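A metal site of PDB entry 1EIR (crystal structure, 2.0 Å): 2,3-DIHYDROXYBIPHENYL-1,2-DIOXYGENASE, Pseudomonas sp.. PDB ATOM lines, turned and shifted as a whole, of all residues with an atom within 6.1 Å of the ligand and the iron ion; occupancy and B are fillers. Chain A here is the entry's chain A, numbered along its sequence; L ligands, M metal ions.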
ATOM      1  N   HIS A 145     -30.332  -0.398 -33.899  1.00  0.00           N
ATOM      2  CA  HIS A 145     -31.128   0.340 -32.928  1.00  0.00           C
ATOM      3  C   HIS A 145     -31.144   1.840 -33.251  1.00  0.00           C
ATOM      4  O   HIS A 145     -30.445   2.300 -34.172  1.00  0.00           O
ATOM      5  CB  HIS A 145     -30.580   0.141 -31.512  1.00  0.00           C
ATOM      6  CG  HIS A 145     -29.356   0.959 -31.202  1.00  0.00           C
ATOM      7  ND1 HIS A 145     -28.106   0.393 -31.044  1.00  0.00           N
ATOM      8  CD2 HIS A 145     -29.195   2.285 -31.009  1.00  0.00           C
ATOM      9  CE1 HIS A 145     -27.238   1.343 -30.765  1.00  0.00           C
ATOM     10  NE2 HIS A 145     -27.872   2.498 -30.742  1.00  0.00           N
ATOM     11  N   VAL A 147     -32.012   5.895 -31.150  1.00  0.00           N
ATOM     12  CA  VAL A 147     -32.365   6.637 -29.945  1.00  0.00           C
ATOM     13  C   VAL A 147     -33.530   7.582 -30.242  1.00  0.00           C
ATOM     14  O   VAL A 147     -33.408   8.493 -31.058  1.00  0.00           O
ATOM     15  CB  VAL A 147     -31.155   7.452 -29.427  1.00  0.00           C
ATOM     16  CG1 VAL A 147     -31.578   8.299 -28.248  1.00  0.00           C
ATOM     17  CG2 VAL A 147     -30.022   6.511 -29.037  1.00  0.00           C
ATOM     18  N   ILE A 172     -28.581   5.294 -18.393  1.00  0.00           N
ATOM     19  CA  ILE A 172     -27.333   6.044 -18.359  1.00  0.00           C
ATOM     20  C   ILE A 172     -27.706   7.500 -18.187  1.00  0.00           C
ATOM     21  O   ILE A 172     -28.571   8.017 -18.906  1.00  0.00           O
ATOM     22  CB  ILE A 172     -26.496   5.910 -19.651  1.00  0.00           C
ATOM     23  CG1 ILE A 172     -26.103   4.441 -19.882  1.00  0.00           C
ATOM     24  CG2 ILE A 172     -25.216   6.764 -19.528  1.00  0.00           C
ATOM     25  CD1 ILE A 172     -25.215   4.230 -21.092  1.00  0.00           C
ATOM     26  N   ILE A 174     -26.823  10.714 -19.038  1.00  0.00           N
ATOM     27  CA  ILE A 174     -25.986  11.415 -19.990  1.00  0.00           C
ATOM     28  C   ILE A 174     -25.875  12.877 -19.591  1.00  0.00           C
ATOM     29  O   ILE A 174     -26.861  13.602 -19.595  1.00  0.00           O
ATOM     30  CB  ILE A 174     -26.559  11.294 -21.418  1.00  0.00           C
ATOM     31  CG1 ILE A 174     -26.646   9.809 -21.802  1.00  0.00           C
ATOM     32  CG2 ILE A 174     -25.680  12.052 -22.395  1.00  0.00           C
ATOM     33  CD1 ILE A 174     -27.463   9.528 -23.047  1.00  0.00           C
ATOM     34  N   ALA A 184     -31.151   8.467 -19.972  1.00  0.00           N
ATOM     35  CA  ALA A 184     -31.473   7.726 -21.188  1.00  0.00           C
ATOM     36  C   ALA A 184     -31.850   6.303 -20.828  1.00  0.00           C
ATOM     37  O   ALA A 184     -31.088   5.631 -20.132  1.00  0.00           O
ATOM     38  CB  ALA A 184     -30.272   7.715 -22.120  1.00  0.00           C
ATOM     39  N   PHE A 186     -32.506   2.509 -22.038  1.00  0.00           N
ATOM     40  CA  PHE A 186     -32.240   1.552 -23.105  1.00  0.00           C
ATOM     41  C   PHE A 186     -33.144   0.331 -22.990  1.00  0.00           C
ATOM     42  O   PHE A 186     -33.234  -0.299 -21.937  1.00  0.00           O
ATOM     43  CB  PHE A 186     -30.757   1.165 -23.082  1.00  0.00           C
ATOM     44  CG  PHE A 186     -29.835   2.343 -23.254  1.00  0.00           C
ATOM     45  CD1 PHE A 186     -29.572   3.191 -22.188  1.00  0.00           C
ATOM     46  CD2 PHE A 186     -29.303   2.642 -24.506  1.00  0.00           C
ATOM     47  CE1 PHE A 186     -28.795   4.340 -22.367  1.00  0.00           C
ATOM     48  CE2 PHE A 186     -28.529   3.784 -24.692  1.00  0.00           C
ATOM     49  CZ  PHE A 186     -28.275   4.633 -23.623  1.00  0.00           C
ATOM     50  N   HIS A 193     -28.503  -5.729 -26.971  1.00  0.00           N
ATOM     51  CA  HIS A 193     -28.582  -4.995 -25.711  1.00  0.00           C
ATOM     52  C   HIS A 193     -29.738  -4.005 -25.721  1.00  0.00           C
ATOM     53  O   HIS A 193     -30.505  -3.921 -24.765  1.00  0.00           O
ATOM     54  CB  HIS A 193     -27.282  -4.249 -25.402  1.00  0.00           C
ATOM     55  CG  HIS A 193     -27.377  -3.408 -24.164  1.00  0.00           C
ATOM     56  ND1 HIS A 193     -27.655  -2.065 -24.201  1.00  0.00           N
ATOM     57  CD2 HIS A 193     -27.295  -3.741 -22.849  1.00  0.00           C
ATOM     58  CE1 HIS A 193     -27.756  -1.602 -22.965  1.00  0.00           C
ATOM     59  NE2 HIS A 193     -27.541  -2.601 -22.128  1.00  0.00           N
ATOM     60  N   HIS A 194     -29.865  -3.249 -26.802  1.00  0.00           N
ATOM     61  CA  HIS A 194     -30.989  -2.330 -26.940  1.00  0.00           C
ATOM     62  C   HIS A 194     -31.312  -2.079 -28.399  1.00  0.00           C
ATOM     63  O   HIS A 194     -30.409  -1.982 -29.247  1.00  0.00           O
ATOM     64  CB  HIS A 194     -30.767  -1.024 -26.160  1.00  0.00           C
ATOM     65  CG  HIS A 194     -29.603  -0.210 -26.639  1.00  0.00           C
ATOM     66  ND1 HIS A 194     -29.755   0.925 -27.406  1.00  0.00           N
ATOM     67  CD2 HIS A 194     -28.269  -0.352 -26.425  1.00  0.00           C
ATOM     68  CE1 HIS A 194     -28.567   1.450 -27.647  1.00  0.00           C
ATOM     69  NE2 HIS A 194     -27.651   0.696 -27.062  1.00  0.00           N
ATOM     70  N   ALA A 197     -33.800   3.292 -27.557  1.00  0.00           N
ATOM     71  CA  ALA A 197     -33.466   4.004 -26.329  1.00  0.00           C
ATOM     72  C   ALA A 197     -34.301   5.278 -26.316  1.00  0.00           C
ATOM     73  O   ALA A 197     -34.502   5.917 -27.350  1.00  0.00           O
ATOM     74  CB  ALA A 197     -31.971   4.331 -26.286  1.00  0.00           C
ATOM     75  N   ALA A 199     -34.771   9.083 -24.606  1.00  0.00           N
ATOM     76  CA  ALA A 199     -34.048  10.141 -23.891  1.00  0.00           C
ATOM     77  C   ALA A 199     -34.657  11.526 -24.159  1.00  0.00           C
ATOM     78  O   ALA A 199     -34.924  11.884 -25.313  1.00  0.00           O
ATOM     79  CB  ALA A 199     -32.569  10.140 -24.298  1.00  0.00           C
ATOM     80  N   PHE A 201     -33.885  14.554 -24.894  1.00  0.00           N
ATOM     81  CA  PHE A 201     -32.857  15.459 -25.398  1.00  0.00           C
ATOM     82  C   PHE A 201     -33.424  16.757 -25.975  1.00  0.00           C
ATOM     83  O   PHE A 201     -34.511  16.771 -26.569  1.00  0.00           O
ATOM     84  CB  PHE A 201     -32.046  14.787 -26.505  1.00  0.00           C
ATOM     85  CG  PHE A 201     -31.068  13.770 -26.011  1.00  0.00           C
ATOM     86  CD1 PHE A 201     -30.771  12.643 -26.772  1.00  0.00           C
ATOM     87  CD2 PHE A 201     -30.427  13.939 -24.774  1.00  0.00           C
ATOM     88  CE1 PHE A 201     -29.842  11.697 -26.324  1.00  0.00           C
ATOM     89  CE2 PHE A 201     -29.504  13.002 -24.316  1.00  0.00           C
ATOM     90  CZ  PHE A 201     -29.215  11.867 -25.097  1.00  0.00           C
ATOM     91  N   HIS A 208     -31.978  10.841 -32.322  1.00  0.00           N
ATOM     92  CA  HIS A 208     -30.653  11.403 -32.147  1.00  0.00           C
ATOM     93  C   HIS A 208     -29.720  10.728 -33.147  1.00  0.00           C
ATOM     94  O   HIS A 208     -28.823  11.355 -33.711  1.00  0.00           O
ATOM     95  CB  HIS A 208     -30.203  11.174 -30.696  1.00  0.00           C
ATOM     96  CG  HIS A 208     -28.791  11.584 -30.432  1.00  0.00           C
ATOM     97  ND1 HIS A 208     -27.722  10.751 -30.699  1.00  0.00           N
ATOM     98  CD2 HIS A 208     -28.267  12.728 -29.953  1.00  0.00           C
ATOM     99  CE1 HIS A 208     -26.597  11.379 -30.390  1.00  0.00           C
ATOM    100  NE2 HIS A 208     -26.903  12.581 -29.929  1.00  0.00           N
ATOM    101  N   HIS A 209     -29.930   9.432 -33.370  1.00  0.00           N
ATOM    102  CA  HIS A 209     -29.130   8.661 -34.318  1.00  0.00           C
ATOM    103  C   HIS A 209     -29.663   7.238 -34.473  1.00  0.00           C
ATOM    104  O   HIS A 209     -30.501   6.789 -33.676  1.00  0.00           O
ATOM    105  CB  HIS A 209     -27.664   8.606 -33.847  1.00  0.00           C
ATOM    106  CG  HIS A 209     -27.426   7.628 -32.735  1.00  0.00           C
ATOM    107  ND1 HIS A 209     -27.390   7.999 -31.408  1.00  0.00           N
ATOM    108  CD2 HIS A 209     -27.228   6.288 -32.746  1.00  0.00           C
ATOM    109  CE1 HIS A 209     -27.187   6.945 -30.647  1.00  0.00           C
ATOM    110  NE2 HIS A 209     -27.085   5.884 -31.441  1.00  0.00           N
ATOM    111  N   PHE A 210     -29.194   6.542 -35.511  1.00  0.00           N
ATOM    112  CA  PHE A 210     -29.551   5.148 -35.722  1.00  0.00           C
ATOM    113  C   PHE A 210     -28.211   4.413 -35.767  1.00  0.00           C
ATOM    114  O   PHE A 210     -27.204   4.995 -36.150  1.00  0.00           O
ATOM    115  CB  PHE A 210     -30.377   4.921 -37.012  1.00  0.00           C
ATOM    116  CG  PHE A 210     -29.598   5.064 -38.298  1.00  0.00           C
ATOM    117  CD1 PHE A 210     -29.149   3.936 -38.985  1.00  0.00           C
ATOM    118  CD2 PHE A 210     -29.362   6.321 -38.848  1.00  0.00           C
ATOM    119  CE1 PHE A 210     -28.487   4.054 -40.199  1.00  0.00           C
ATOM    120  CE2 PHE A 210     -28.700   6.460 -40.070  1.00  0.00           C
ATOM    121  CZ  PHE A 210     -28.261   5.318 -40.754  1.00  0.00           C
ATOM    122  N   MET A 211     -28.203   3.157 -35.340  1.00  0.00           N
ATOM    123  CA  MET A 211     -26.953   2.403 -35.300  1.00  0.00           C
ATOM    124  C   MET A 211     -26.924   1.118 -36.132  1.00  0.00           C
ATOM    125  O   MET A 211     -27.919   0.403 -36.219  1.00  0.00           O
ATOM    126  CB  MET A 211     -26.620   2.065 -33.839  1.00  0.00           C
ATOM    127  CG  MET A 211     -25.301   1.325 -33.636  1.00  0.00           C
ATOM    128  SD  MET A 211     -25.497  -0.483 -33.658  1.00  0.00           S
ATOM    129  CE  MET A 211     -23.824  -0.989 -33.223  1.00  0.00           C
ATOM    130  N   HIS A 240     -18.927   1.647 -25.290  1.00  0.00           N
ATOM    131  CA  HIS A 240     -19.970   2.036 -24.350  1.00  0.00           C
ATOM    132  C   HIS A 240     -19.882   1.291 -23.016  1.00  0.00           C
ATOM    133  O   HIS A 240     -19.304   0.208 -22.918  1.00  0.00           O
ATOM    134  CB  HIS A 240     -21.345   1.819 -24.981  1.00  0.00           C
ATOM    135  CG  HIS A 240     -21.671   2.800 -26.071  1.00  0.00           C
ATOM    136  ND1 HIS A 240     -21.771   4.149 -25.840  1.00  0.00           N
ATOM    137  CD2 HIS A 240     -21.902   2.620 -27.384  1.00  0.00           C
ATOM    138  CE1 HIS A 240     -22.061   4.767 -26.969  1.00  0.00           C
ATOM    139  NE2 HIS A 240     -22.156   3.854 -27.926  1.00  0.00           N
ATOM    140  N   THR A 241     -20.475   1.905 -21.998  1.00  0.00           N
ATOM    141  CA  THR A 241     -20.508   1.351 -20.653  1.00  0.00           C
ATOM    142  C   THR A 241     -21.534   0.222 -20.522  1.00  0.00           C
ATOM    143  O   THR A 241     -21.256  -0.810 -19.924  1.00  0.00           O
ATOM    144  CB  THR A 241     -20.885   2.451 -19.622  1.00  0.00           C
ATOM    145  OG1 THR A 241     -22.046   3.163 -20.067  1.00  0.00           O
ATOM    146  CG2 THR A 241     -19.730   3.439 -19.417  1.00  0.00           C
ATOM    147  N   ASN A 242     -22.709   0.425 -21.102  1.00  0.00           N
ATOM    148  CA  ASN A 242     -23.776  -0.568 -21.016  1.00  0.00           C
ATOM    149  C   ASN A 242     -23.771  -1.723 -22.026  1.00  0.00           C
ATOM    150  O   ASN A 242     -23.810  -2.890 -21.617  1.00  0.00           O
ATOM    151  CB  ASN A 242     -25.145   0.130 -21.012  1.00  0.00           C
ATOM    152  CG  ASN A 242     -25.402   0.955 -22.275  1.00  0.00           C
ATOM    153  OD1 ASN A 242     -24.511   1.168 -23.109  1.00  0.00           O
ATOM    154  ND2 ASN A 242     -26.638   1.421 -22.419  1.00  0.00           N
ATOM    155  N   ASP A 243     -23.716  -1.445 -23.327  1.00  0.00           N
ATOM    156  CA  ASP A 243     -23.721  -2.532 -24.300  1.00  0.00           C
ATOM    157  C   ASP A 243     -22.330  -2.995 -24.698  1.00  0.00           C
ATOM    158  O   ASP A 243     -22.184  -4.033 -25.343  1.00  0.00           O
ATOM    159  CB  ASP A 243     -24.534  -2.165 -25.555  1.00  0.00           C
ATOM    160  CG  ASP A 243     -23.872  -1.090 -26.411  1.00  0.00           C
ATOM    161  OD1 ASP A 243     -24.533  -0.576 -27.344  1.00  0.00           O
ATOM    162  OD2 ASP A 243     -22.689  -0.744 -26.168  1.00  0.00           O
ATOM    163  N   THR A 245     -20.406  -1.803 -26.851  1.00  0.00           N
ATOM    164  CA  THR A 245     -20.240  -1.705 -28.287  1.00  0.00           C
ATOM    165  C   THR A 245     -19.027  -0.804 -28.533  1.00  0.00           C
ATOM    166  O   THR A 245     -18.832   0.190 -27.840  1.00  0.00           O
ATOM    167  CB  THR A 245     -21.487  -1.075 -28.953  1.00  0.00           C
ATOM    168  OG1 THR A 245     -22.543  -2.044 -29.000  1.00  0.00           O
ATOM    169  CG2 THR A 245     -21.167  -0.620 -30.386  1.00  0.00           C
ATOM    170  N   SER A 247     -17.599   1.605 -31.120  1.00  0.00           N
ATOM    171  CA  SER A 247     -18.048   2.335 -32.288  1.00  0.00           C
ATOM    172  C   SER A 247     -17.549   3.770 -32.362  1.00  0.00           C
ATOM    173  O   SER A 247     -16.703   4.208 -31.585  1.00  0.00           O
ATOM    174  CB  SER A 247     -19.574   2.372 -32.279  1.00  0.00           C
ATOM    175  OG  SER A 247     -20.042   2.934 -31.062  1.00  0.00           O
ATOM    176  N   TYR A 249     -19.205   7.815 -34.020  1.00  0.00           N
ATOM    177  CA  TYR A 249     -20.393   8.481 -34.529  1.00  0.00           C
ATOM    178  C   TYR A 249     -20.025   9.396 -35.686  1.00  0.00           C
ATOM    179  O   TYR A 249     -18.862   9.797 -35.829  1.00  0.00           O
ATOM    180  CB  TYR A 249     -21.068   9.283 -33.416  1.00  0.00           C
ATOM    181  CG  TYR A 249     -21.659   8.421 -32.310  1.00  0.00           C
ATOM    182  CD1 TYR A 249     -23.036   8.230 -32.214  1.00  0.00           C
ATOM    183  CD2 TYR A 249     -20.850   7.847 -31.328  1.00  0.00           C
ATOM    184  CE1 TYR A 249     -23.599   7.503 -31.170  1.00  0.00           C
ATOM    185  CE2 TYR A 249     -21.391   7.125 -30.284  1.00  0.00           C
ATOM    186  CZ  TYR A 249     -22.759   6.953 -30.200  1.00  0.00           C
ATOM    187  OH  TYR A 249     -23.302   6.261 -29.142  1.00  0.00           O
ATOM    188  N   GLU A 260     -24.310   5.681 -35.955  1.00  0.00           N
ATOM    189  CA  GLU A 260     -23.297   5.022 -35.153  1.00  0.00           C
ATOM    190  C   GLU A 260     -22.948   3.710 -35.849  1.00  0.00           C
ATOM    191  O   GLU A 260     -23.810   2.928 -36.235  1.00  0.00           O
ATOM    192  CB  GLU A 260     -23.813   4.763 -33.743  1.00  0.00           C
ATOM    193  CG  GLU A 260     -22.723   4.301 -32.791  1.00  0.00           C
ATOM    194  CD  GLU A 260     -23.256   3.889 -31.435  1.00  0.00           C
ATOM    195  OE1 GLU A 260     -24.483   3.853 -31.272  1.00  0.00           O
ATOM    196  OE2 GLU A 260     -22.444   3.622 -30.529  1.00  0.00           O
ATOM    197  N   THR A 280     -21.573   7.324 -20.821  1.00  0.00           N
ATOM    198  CA  THR A 280     -22.001   6.527 -21.982  1.00  0.00           C
ATOM    199  C   THR A 280     -20.832   5.738 -22.534  1.00  0.00           C
ATOM    200  O   THR A 280     -21.018   4.814 -23.316  1.00  0.00           O
ATOM    201  CB  THR A 280     -22.569   7.398 -23.146  1.00  0.00           C
ATOM    202  OG1 THR A 280     -21.561   8.317 -23.590  1.00  0.00           O
ATOM    203  CG2 THR A 280     -23.831   8.142 -22.724  1.00  0.00           C
HETATM  204  C1  LIG L   1     -25.261   5.359 -24.853  1.00  0.00           C
HETATM  205  C2  LIG L   1     -25.558   5.788 -26.210  1.00  0.00           C
HETATM  206  C3  LIG L   1     -25.562   4.828 -27.287  1.00  0.00           C
HETATM  207  C4  LIG L   1     -25.286   3.433 -27.023  1.00  0.00           C
HETATM  208  C5  LIG L   1     -24.992   2.997 -25.671  1.00  0.00           C
HETATM  209  C6  LIG L   1     -24.976   3.963 -24.592  1.00  0.00           C
HETATM  210  C7  LIG L   1     -25.851   7.156 -26.483  1.00  0.00           C
HETATM  211  C8  LIG L   1     -27.219   7.568 -26.742  1.00  0.00           C
HETATM  212  C9  LIG L   1     -27.509   8.962 -27.047  1.00  0.00           C
HETATM  213  C10 LIG L   1     -26.433   9.935 -27.098  1.00  0.00           C
HETATM  214  C11 LIG L   1     -25.057   9.528 -26.849  1.00  0.00           C
HETATM  215  C12 LIG L   1     -24.764   8.142 -26.538  1.00  0.00           C
HETATM  216  O1  LIG L   1     -25.270   2.531 -28.064  1.00  0.00           O
HETATM  217  O2  LIG L   1     -25.825   5.238 -28.573  1.00  0.00           O
HETATM  218 FE    FE M   1     -26.330   4.109 -30.050  1.00  0.00          FE
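An oxygen (O2) of the ligand sits close to the side-chain hydroxyl (OH) of Tyr 249 (2.8 Å).
An oxygen (O1) of the ligand is in hydrogen-bond range of the side-chain carboxylate (OD1) of Asp 243 (3.3 Å).
O1 of the ligand sits at hydrogen-bond distance from NE2 of His 194 (3.2 Å).
NE2 of His 240 lies close to O1 of the ligand (3.4 Å).
The side-chain hydroxyl (OH) of Tyr 249 lies close to a ring nitrogen (NE2) of His 240, 2.9 Å away.
The backbone NH (N) of His 208 is in hydrogen-bond range of the backbone carbonyl oxygen (O) of Val 147 (3.0 Å).
The backbone NH (N) of Met 211 is in hydrogen-bond range of the backbone carbonyl oxygen (O) of His 145, 2.7 Å away.
A ring nitrogen (ND1) of His 240 sits at hydrogen-bond distance from the backbone carbonyl oxygen (O) of Thr 280, at 2.7 Å.
The backbone NH (N) of Glu 260 lies within hydrogen-bond range of the backbone carbonyl oxygen (O) of Phe 210 (3.0 Å).
The backbone carbonyl oxygen of Ile 172 sits at hydrogen-bond distance from the backbone NH of Ala 184 (2.8 Å).
ND1 of His 209 lies within hydrogen-bond range of ND1 of His 208 (2.9 Å).
N of Val 147 lies within hydrogen-bond range of O of His 209 (3.1 Å).
Val 147 touches the ligand.
Ile 172 touches the ligand (CD1 to C6, 3.5 Å).
Phe 186 touches the ligand (CZ to C1, 3.3 Å).
Phe 201 touches the ligand.
His 208 touches the ligand (CE1 to C10, 3.6 Å).
Asn 242 touches the ligand.
Thr 280 touches the ligand (CB to C1, 3.8 Å).
Merely in contact with the iron ion: Tyr 249 (3.8 Å).
Of the 24 residues printed, 4 come within 4 Å of the iron ion.
The nearest printed residue that does not touch the iron ion is His 194 (4.2 Å).
The iron ion is bound by an oxygen (O2) of the ligand (1.9 Å), the side-chain carboxylate (OE1) of Glu 260 (2.2 Å), a ring nitrogen (NE2) of His 145 (2.3 Å) and a ring nitrogen (NE2) of His 209 (2.4 Å).
The iron ion has four donor atoms within binding distance.
Slightly farther from the iron ion lies O1 of the ligand (2.7 Å).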
